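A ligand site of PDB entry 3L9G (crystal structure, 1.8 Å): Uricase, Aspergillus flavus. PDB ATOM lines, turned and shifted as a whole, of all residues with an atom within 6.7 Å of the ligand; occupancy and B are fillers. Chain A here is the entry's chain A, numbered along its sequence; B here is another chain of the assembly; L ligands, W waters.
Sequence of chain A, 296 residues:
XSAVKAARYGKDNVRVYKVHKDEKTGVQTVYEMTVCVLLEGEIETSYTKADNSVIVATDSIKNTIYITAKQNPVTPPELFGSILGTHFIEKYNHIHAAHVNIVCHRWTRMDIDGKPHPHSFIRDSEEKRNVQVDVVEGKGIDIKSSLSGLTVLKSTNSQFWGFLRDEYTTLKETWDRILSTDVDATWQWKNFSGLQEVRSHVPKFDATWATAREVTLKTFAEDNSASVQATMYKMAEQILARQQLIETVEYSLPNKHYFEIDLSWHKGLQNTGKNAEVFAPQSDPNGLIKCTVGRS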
ATOM      1  N   SER A 158      14.760 -17.233  -4.387  1.00  0.00           N
ATOM      2  CA  SER A 158      13.741 -17.877  -3.580  1.00  0.00           C
ATOM      3  C   SER A 158      14.471 -18.643  -2.477  1.00  0.00           C
ATOM      4  O   SER A 158      15.460 -19.310  -2.756  1.00  0.00           O
ATOM      5  CB  SER A 158      12.817 -18.785  -4.380  1.00  0.00           C
ATOM      6  OG  SER A 158      11.896 -19.482  -3.536  1.00  0.00           O
ATOM      7  N   GLN A 159      13.976 -18.543  -1.246  1.00  0.00           N
ATOM      8  CA  GLN A 159      14.557 -19.193  -0.103  1.00  0.00           C
ATOM      9  C   GLN A 159      13.475 -19.866   0.725  1.00  0.00           C
ATOM     10  O   GLN A 159      12.309 -19.493   0.638  1.00  0.00           O
ATOM     11  CB  GLN A 159      15.326 -18.184   0.755  1.00  0.00           C
ATOM     12  CG  GLN A 159      16.316 -17.349  -0.054  1.00  0.00           C
ATOM     13  CD  GLN A 159      17.023 -16.347   0.864  1.00  0.00           C
ATOM     14  OE1 GLN A 159      17.457 -16.686   1.955  1.00  0.00           O
ATOM     15  NE2 GLN A 159      17.115 -15.114   0.392  1.00  0.00           N
ATOM     16  N   PHE A 160      13.851 -20.848   1.521  1.00  0.00           N
ATOM     17  CA  PHE A 160      12.892 -21.425   2.465  1.00  0.00           C
ATOM     18  C   PHE A 160      13.669 -22.078   3.605  1.00  0.00           C
ATOM     19  O   PHE A 160      14.183 -23.199   3.536  1.00  0.00           O
ATOM     20  CB  PHE A 160      11.895 -22.394   1.803  1.00  0.00           C
ATOM     21  CG  PHE A 160      10.749 -22.727   2.753  1.00  0.00           C
ATOM     22  CD1 PHE A 160       9.886 -21.706   3.152  1.00  0.00           C
ATOM     23  CD2 PHE A 160      10.535 -23.992   3.253  1.00  0.00           C
ATOM     24  CE1 PHE A 160       8.852 -21.944   4.030  1.00  0.00           C
ATOM     25  CE2 PHE A 160       9.484 -24.244   4.130  1.00  0.00           C
ATOM     26  CZ  PHE A 160       8.637 -23.222   4.524  1.00  0.00           C
ATOM     27  N   PHE A 163      11.766 -22.816   9.142  1.00  0.00           N
ATOM     28  CA  PHE A 163      10.448 -23.365   9.396  1.00  0.00           C
ATOM     29  C   PHE A 163      10.505 -24.348  10.557  1.00  0.00           C
ATOM     30  O   PHE A 163      11.610 -24.731  10.940  1.00  0.00           O
ATOM     31  CB  PHE A 163       9.874 -24.042   8.149  1.00  0.00           C
ATOM     32  CG  PHE A 163      10.894 -24.967   7.484  1.00  0.00           C
ATOM     33  CD1 PHE A 163      11.748 -24.506   6.510  1.00  0.00           C
ATOM     34  CD2 PHE A 163      10.961 -26.310   7.840  1.00  0.00           C
ATOM     35  CE1 PHE A 163      12.652 -25.326   5.871  1.00  0.00           C
ATOM     36  CE2 PHE A 163      11.875 -27.143   7.214  1.00  0.00           C
ATOM     37  CZ  PHE A 163      12.722 -26.653   6.245  1.00  0.00           C
ATOM     38  N   LEU A 171      12.757 -32.078   5.485  1.00  0.00           N
ATOM     39  CA  LEU A 171      13.139 -31.128   4.465  1.00  0.00           C
ATOM     40  C   LEU A 171      14.356 -30.333   4.903  1.00  0.00           C
ATOM     41  O   LEU A 171      14.356 -29.783   6.015  1.00  0.00           O
ATOM     42  CB  LEU A 171      11.972 -30.180   4.212  1.00  0.00           C
ATOM     43  CG  LEU A 171      12.225 -29.013   3.248  1.00  0.00           C
ATOM     44  CD1 LEU A 171      12.333 -29.525   1.824  1.00  0.00           C
ATOM     45  CD2 LEU A 171      11.137 -27.960   3.342  1.00  0.00           C
ATOM     46  N   ARG A 177      16.721 -21.596  -4.048  1.00  0.00           N
ATOM     47  CA  ARG A 177      15.943 -22.627  -4.717  1.00  0.00           C
ATOM     48  C   ARG A 177      15.221 -22.008  -5.908  1.00  0.00           C
ATOM     49  O   ARG A 177      15.166 -20.787  -6.092  1.00  0.00           O
ATOM     50  CB  ARG A 177      14.962 -23.277  -3.741  1.00  0.00           C
ATOM     51  CG  ARG A 177      13.833 -22.332  -3.332  1.00  0.00           C
ATOM     52  CD  ARG A 177      12.858 -22.921  -2.337  1.00  0.00           C
ATOM     53  NE  ARG A 177      11.729 -22.018  -2.151  1.00  0.00           N
ATOM     54  CZ  ARG A 177      10.618 -22.290  -1.491  1.00  0.00           C
ATOM     55  NH1 ARG A 177      10.430 -23.461  -0.903  1.00  0.00           N
ATOM     56  NH2 ARG A 177       9.669 -21.363  -1.410  1.00  0.00           N
ATOM     57  N   LEU A 179      11.644 -21.232  -7.685  1.00  0.00           N
ATOM     58  CA  LEU A 179      10.233 -21.073  -7.353  1.00  0.00           C
ATOM     59  C   LEU A 179       9.404 -20.957  -8.615  1.00  0.00           C
ATOM     60  O   LEU A 179       9.637 -20.103  -9.479  1.00  0.00           O
ATOM     61  CB  LEU A 179      10.010 -19.846  -6.466  1.00  0.00           C
ATOM     62  CG  LEU A 179       8.552 -19.479  -6.157  1.00  0.00           C
ATOM     63  CD1 LEU A 179       7.868 -20.586  -5.385  1.00  0.00           C
ATOM     64  CD2 LEU A 179       8.486 -18.181  -5.378  1.00  0.00           C
ATOM     65  N   SER A 225      12.523 -14.040  -2.172  1.00  0.00           N
ATOM     66  CA  SER A 225      11.394 -14.599  -1.440  1.00  0.00           C
ATOM     67  C   SER A 225      11.725 -15.463  -0.247  1.00  0.00           C
ATOM     68  O   SER A 225      12.494 -16.419  -0.360  1.00  0.00           O
ATOM     69  CB  SER A 225      10.570 -15.424  -2.455  1.00  0.00           C
ATOM     70  OG  SER A 225       9.633 -16.251  -1.763  1.00  0.00           O
ATOM     71  N   ALA A 226      11.126 -15.140   0.907  1.00  0.00           N
ATOM     72  CA  ALA A 226      11.308 -15.848   2.156  1.00  0.00           C
ATOM     73  C   ALA A 226      10.457 -17.113   2.198  1.00  0.00           C
ATOM     74  O   ALA A 226      10.757 -18.044   2.946  1.00  0.00           O
ATOM     75  CB  ALA A 226      10.936 -14.967   3.348  1.00  0.00           C
ATOM     76  N   SER A 227       9.407 -17.063   1.384  1.00  0.00           N
ATOM     77  CA  SER A 227       8.407 -18.104   1.272  1.00  0.00           C
ATOM     78  C   SER A 227       7.333 -17.671   0.277  1.00  0.00           C
ATOM     79  O   SER A 227       7.226 -16.485  -0.007  1.00  0.00           O
ATOM     80  CB  SER A 227       7.748 -18.463   2.594  1.00  0.00           C
ATOM     81  OG  SER A 227       6.943 -17.441   3.103  1.00  0.00           O
ATOM     82  N   VAL A 228       6.558 -18.628  -0.213  1.00  0.00           N
ATOM     83  CA  VAL A 228       5.410 -18.292  -1.035  1.00  0.00           C
ATOM     84  C   VAL A 228       4.444 -17.387  -0.262  1.00  0.00           C
ATOM     85  O   VAL A 228       3.987 -16.368  -0.801  1.00  0.00           O
ATOM     86  CB  VAL A 228       4.704 -19.545  -1.567  1.00  0.00           C
ATOM     87  CG1 VAL A 228       3.499 -19.122  -2.396  1.00  0.00           C
ATOM     88  CG2 VAL A 228       5.621 -20.400  -2.425  1.00  0.00           C
ATOM     89  N   GLN A 229       4.139 -17.740   0.974  1.00  0.00           N
ATOM     90  CA  GLN A 229       3.327 -16.928   1.880  1.00  0.00           C
ATOM     91  C   GLN A 229       3.714 -15.455   1.887  1.00  0.00           C
ATOM     92  O   GLN A 229       2.869 -14.572   1.728  1.00  0.00           O
ATOM     93  CB  GLN A 229       3.472 -17.500   3.285  1.00  0.00           C
ATOM     94  CG  GLN A 229       2.797 -18.815   3.602  1.00  0.00           C
ATOM     95  CD  GLN A 229       3.637 -20.041   3.301  1.00  0.00           C
ATOM     96  OE1 GLN A 229       4.514 -20.032   2.432  1.00  0.00           O
ATOM     97  NE2 GLN A 229       3.327 -21.125   4.001  1.00  0.00           N
ATOM     98  N   ASN A 255       3.016 -24.484  -5.067  1.00  0.00           N
ATOM     99  CA  ASN A 255       4.479 -24.479  -5.142  1.00  0.00           C
ATOM    100  C   ASN A 255       4.829 -25.713  -5.978  1.00  0.00           C
ATOM    101  O   ASN A 255       4.702 -26.834  -5.465  1.00  0.00           O
ATOM    102  CB  ASN A 255       5.100 -24.510  -3.778  1.00  0.00           C
ATOM    103  CG  ASN A 255       6.585 -24.175  -3.729  1.00  0.00           C
ATOM    104  OD1 ASN A 255       7.207 -23.929  -4.744  1.00  0.00           O
ATOM    105  ND2 ASN A 255       7.116 -24.154  -2.513  1.00  0.00           N
ATOM    106  N   HIS A 257       7.229 -27.936  -7.307  1.00  0.00           N
ATOM    107  CA  HIS A 257       8.571 -28.241  -6.861  1.00  0.00           C
ATOM    108  C   HIS A 257       9.500 -28.704  -7.962  1.00  0.00           C
ATOM    109  O   HIS A 257       9.182 -29.474  -8.850  1.00  0.00           O
ATOM    110  CB  HIS A 257       8.531 -29.339  -5.790  1.00  0.00           C
ATOM    111  CG  HIS A 257       7.654 -29.002  -4.623  1.00  0.00           C
ATOM    112  ND1 HIS A 257       7.781 -27.857  -3.889  1.00  0.00           N
ATOM    113  CD2 HIS A 257       6.606 -29.684  -4.082  1.00  0.00           C
ATOM    114  CE1 HIS A 257       6.847 -27.845  -2.935  1.00  0.00           C
ATOM    115  NE2 HIS A 257       6.126 -28.950  -3.031  1.00  0.00           N
ATOM    116  N   GLY A 287       2.981 -28.096  -2.980  1.00  0.00           N
ATOM    117  CA  GLY A 287       2.438 -27.190  -1.978  1.00  0.00           C
ATOM    118  C   GLY A 287       1.283 -26.413  -2.589  1.00  0.00           C
ATOM    119  O   GLY A 287       1.229 -26.172  -3.794  1.00  0.00           O
ATOM    120  N   ILE A 289      -0.729 -22.866  -1.319  1.00  0.00           N
ATOM    121  CA  ILE A 289      -0.601 -21.762  -0.364  1.00  0.00           C
ATOM    122  C   ILE A 289      -1.702 -20.748  -0.710  1.00  0.00           C
ATOM    123  O   ILE A 289      -1.797 -20.327  -1.852  1.00  0.00           O
ATOM    124  CB  ILE A 289       0.803 -21.162  -0.404  1.00  0.00           C
ATOM    125  CG1 ILE A 289       1.970 -22.154  -0.424  1.00  0.00           C
ATOM    126  CG2 ILE A 289       1.047 -20.192   0.750  1.00  0.00           C
ATOM    127  CD1 ILE A 289       1.944 -23.168   0.682  1.00  0.00           C
ATOM    128  N   TYR B   9      -2.812 -23.302   4.155  1.00  0.00           N
ATOM    129  CA  TYR B   9      -1.694 -23.721   3.318  1.00  0.00           C
ATOM    130  C   TYR B   9      -1.437 -25.205   3.620  1.00  0.00           C
ATOM    131  O   TYR B   9      -1.800 -25.701   4.702  1.00  0.00           O
ATOM    132  CB  TYR B   9      -0.444 -22.848   3.559  1.00  0.00           C
ATOM    133  CG  TYR B   9       0.318 -23.436   4.728  1.00  0.00           C
ATOM    134  CD1 TYR B   9      -0.238 -23.267   5.999  1.00  0.00           C
ATOM    135  CD2 TYR B   9       1.493 -24.156   4.574  1.00  0.00           C
ATOM    136  CE1 TYR B   9       0.396 -23.778   7.114  1.00  0.00           C
ATOM    137  CE2 TYR B   9       2.119 -24.677   5.678  1.00  0.00           C
ATOM    138  CZ  TYR B   9       1.565 -24.488   6.938  1.00  0.00           C
ATOM    139  OH  TYR B   9       2.186 -25.019   8.044  1.00  0.00           O
ATOM    140  N   GLY B  10      -0.787 -25.877   2.695  1.00  0.00           N
ATOM    141  CA  GLY B  10      -0.401 -27.259   2.905  1.00  0.00           C
ATOM    142  C   GLY B  10       0.021 -27.966   1.636  1.00  0.00           C
ATOM    143  O   GLY B  10       0.565 -27.323   0.751  1.00  0.00           O
ATOM    144  N   LYS B  11      -0.245 -29.281   1.588  1.00  0.00           N
ATOM    145  CA  LYS B  11       0.202 -30.124   0.467  1.00  0.00           C
ATOM    146  C   LYS B  11      -1.037 -30.691  -0.238  1.00  0.00           C
ATOM    147  O   LYS B  11      -1.899 -31.207   0.452  1.00  0.00           O
ATOM    148  CB  LYS B  11       1.119 -31.266   0.915  1.00  0.00           C
ATOM    149  CG  LYS B  11       1.920 -31.858  -0.259  1.00  0.00           C
ATOM    150  CD  LYS B  11       2.994 -30.912  -0.776  1.00  0.00           C
ATOM    151  CE  LYS B  11       4.381 -31.185  -0.258  1.00  0.00           C
ATOM    152  NZ  LYS B  11       5.377 -30.140  -0.580  1.00  0.00           N
ATOM    153  N   ASN B  52       8.920 -17.760   9.245  1.00  0.00           N
ATOM    154  CA  ASN B  52       8.690 -19.167   8.909  1.00  0.00           C
ATOM    155  C   ASN B  52       8.588 -20.065  10.110  1.00  0.00           C
ATOM    156  O   ASN B  52       8.161 -21.229   9.996  1.00  0.00           O
ATOM    157  CB  ASN B  52       9.778 -19.658   7.929  1.00  0.00           C
ATOM    158  CG  ASN B  52       9.545 -19.076   6.559  1.00  0.00           C
ATOM    159  OD1 ASN B  52       8.478 -18.570   6.227  1.00  0.00           O
ATOM    160  ND2 ASN B  52      10.560 -19.134   5.718  1.00  0.00           N
ATOM    161  N   ILE B  55       5.496 -22.063  10.431  1.00  0.00           N
ATOM    162  CA  ILE B  55       5.108 -22.958   9.344  1.00  0.00           C
ATOM    163  C   ILE B  55       5.548 -24.394   9.632  1.00  0.00           C
ATOM    164  O   ILE B  55       6.718 -24.712   9.753  1.00  0.00           O
ATOM    165  CB  ILE B  55       5.675 -22.498   7.998  1.00  0.00           C
ATOM    166  CG1 ILE B  55       5.171 -21.126   7.531  1.00  0.00           C
ATOM    167  CG2 ILE B  55       5.401 -23.518   6.896  1.00  0.00           C
ATOM    168  CD1 ILE B  55       6.015 -20.569   6.389  1.00  0.00           C
ATOM    169  N   VAL B  56       4.543 -25.276   9.693  1.00  0.00           N
ATOM    170  CA  VAL B  56       4.780 -26.705   9.587  1.00  0.00           C
ATOM    171  C   VAL B  56       4.959 -26.963   8.075  1.00  0.00           C
ATOM    172  O   VAL B  56       3.979 -26.787   7.342  1.00  0.00           O
ATOM    173  CB  VAL B  56       3.613 -27.542  10.101  1.00  0.00           C
ATOM    174  CG1 VAL B  56       3.851 -29.020   9.869  1.00  0.00           C
ATOM    175  CG2 VAL B  56       3.362 -27.287  11.586  1.00  0.00           C
ATOM    176  N   ALA B  57       6.172 -27.298   7.658  1.00  0.00           N
ATOM    177  CA  ALA B  57       6.474 -27.423   6.228  1.00  0.00           C
ATOM    178  C   ALA B  57       5.469 -28.303   5.494  1.00  0.00           C
ATOM    179  O   ALA B  57       5.083 -29.355   6.001  1.00  0.00           O
ATOM    180  CB  ALA B  57       7.857 -27.982   6.005  1.00  0.00           C
ATOM    181  N   THR B  58       5.058 -27.894   4.283  1.00  0.00           N
ATOM    182  CA  THR B  58       4.160 -28.737   3.510  1.00  0.00           C
ATOM    183  C   THR B  58       4.818 -30.076   3.213  1.00  0.00           C
ATOM    184  O   THR B  58       4.113 -31.077   3.141  1.00  0.00           O
ATOM    185  CB  THR B  58       3.659 -28.081   2.215  1.00  0.00           C
ATOM    186  OG1 THR B  58       4.703 -27.972   1.237  1.00  0.00           O
ATOM    187  CG2 THR B  58       3.179 -26.653   2.469  1.00  0.00           C
ATOM    188  N   ASP B  59       6.146 -30.111   3.110  1.00  0.00           N
ATOM    189  CA  ASP B  59       6.848 -31.370   2.959  1.00  0.00           C
ATOM    190  C   ASP B  59       6.651 -32.242   4.193  1.00  0.00           C
ATOM    191  O   ASP B  59       6.496 -33.449   4.080  1.00  0.00           O
ATOM    192  CB  ASP B  59       8.358 -31.164   2.736  1.00  0.00           C
ATOM    193  CG  ASP B  59       9.066 -32.448   2.396  1.00  0.00           C
ATOM    194  OD1 ASP B  59       9.032 -32.857   1.218  1.00  0.00           O
ATOM    195  OD2 ASP B  59       9.673 -33.052   3.304  1.00  0.00           O
ATOM    196  N   SER B  60       6.681 -31.629   5.376  1.00  0.00           N
ATOM    197  CA  SER B  60       6.361 -32.368   6.590  1.00  0.00           C
ATOM    198  C   SER B  60       4.908 -32.805   6.659  1.00  0.00           C
ATOM    199  O   SER B  60       4.584 -33.879   7.162  1.00  0.00           O
ATOM    200  CB  SER B  60       6.721 -31.468   7.801  1.00  0.00           C
ATOM    201  OG  SER B  60       8.060 -31.013   7.667  1.00  0.00           O
HETATM  202  N1  LIG L   1       6.174 -22.471   1.878  1.00  0.00           N
HETATM  203  C1  LIG L   1       7.209 -22.376   0.956  1.00  0.00           C
HETATM  204  C2  LIG L   1       5.831 -23.569   2.631  1.00  0.00           C
HETATM  205  N2  LIG L   1       7.954 -23.486   0.674  1.00  0.00           N
HETATM  206  O1  LIG L   1       7.427 -21.337   0.374  1.00  0.00           O
HETATM  207  C3  LIG L   1       7.635 -24.601   1.373  1.00  0.00           C
HETATM  208  C4  LIG L   1       6.623 -24.716   2.308  1.00  0.00           C
HETATM  209  N3  LIG L   1       8.183 -25.849   1.258  1.00  0.00           N
HETATM  210  O2  LIG L   1       4.921 -23.507   3.439  1.00  0.00           O
HETATM  211  N4  LIG L   1       6.589 -25.933   2.829  1.00  0.00           N
HETATM  212  C5  LIG L   1       7.527 -26.700   2.151  1.00  0.00           C
HETATM  213  O3  LIG L   1       7.803 -27.920   2.266  1.00  0.00           O
HETATM  214  O   HOH W   1      10.000 -26.753  -0.863  1.00  0.00           O
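The guanidinium group (NH2) of Arg 177 sits at hydrogen-bond distance from an oxygen (O1) of the ligand.
The backbone NH (N) of Asp 59 of chain B lies within hydrogen-bond range of an oxygen (O3) of the ligand (2.9 Å).
N of Thr 58 of chain B is in hydrogen-bond range of O3 of the ligand, 3.4 Å away.
The side-chain hydroxyl (OG1) of Thr 58 of chain B lies within hydrogen-bond range of a nitrogen (N4) of the ligand.
N of Val 228 is in hydrogen-bond range of O1 of the ligand, 2.9 Å away.
The side-chain amide nitrogen (NE2) of Gln 229 sits at hydrogen-bond distance from an oxygen (O2) of the ligand.
N2 of the ligand lies close to ND2 of Asn 255 (3.4 Å).
The guanidinium group (NE) of Arg 177 is in hydrogen-bond range of the side-chain hydroxyl (OG) of Ser 158, at 2.9 Å.
The side-chain amino group of Lys 11 of chain B sits at hydrogen-bond distance from the side-chain hydroxyl of Thr 58 of chain B (2.9 Å).
The backbone carbonyl oxygen (O) of Gly 287 is in hydrogen-bond range of the backbone NH (N) of Asn 255, at 2.8 Å.
The backbone carbonyl oxygen (O) of Ser 227 sits at hydrogen-bond distance from the side-chain hydroxyl (OG) of Ser 225 (3.0 Å).
The backbone carbonyl oxygen of Val 56 of chain B is in hydrogen-bond range of the side-chain hydroxyl of Tyr 9 of chain B, at 2.6 Å.
Phe 160 touches the ligand.
CD2 of Leu 171 touches O3 of the ligand, at 3.5 Å.
Ser 227 touches the ligand.
CD2 of Tyr 9 of chain B touches O2 of the ligand, at 3.7 Å.
Ile 55 of chain B touches the ligand (CG2 to O2, 3.5 Å).
Ala 57 of chain B touches the ligand (CA to N4, 3.7 Å).
Hydrophobic or aromatic side chains within 4 Å of the ligand: Phe 160, Leu 171, Val 228, Tyr 9 of chain B, Ile 55 of chain B and Ala 57 of chain B.
Along chain A the residues within 4 Å of the ligand span positions 160 to 255.
The nearest printed residue that does not touch the ligand is Ile 289 (4.1 Å).
Water W1 lies within hydrogen-bond range of N3 of the ligand and NH1 of Arg 177.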
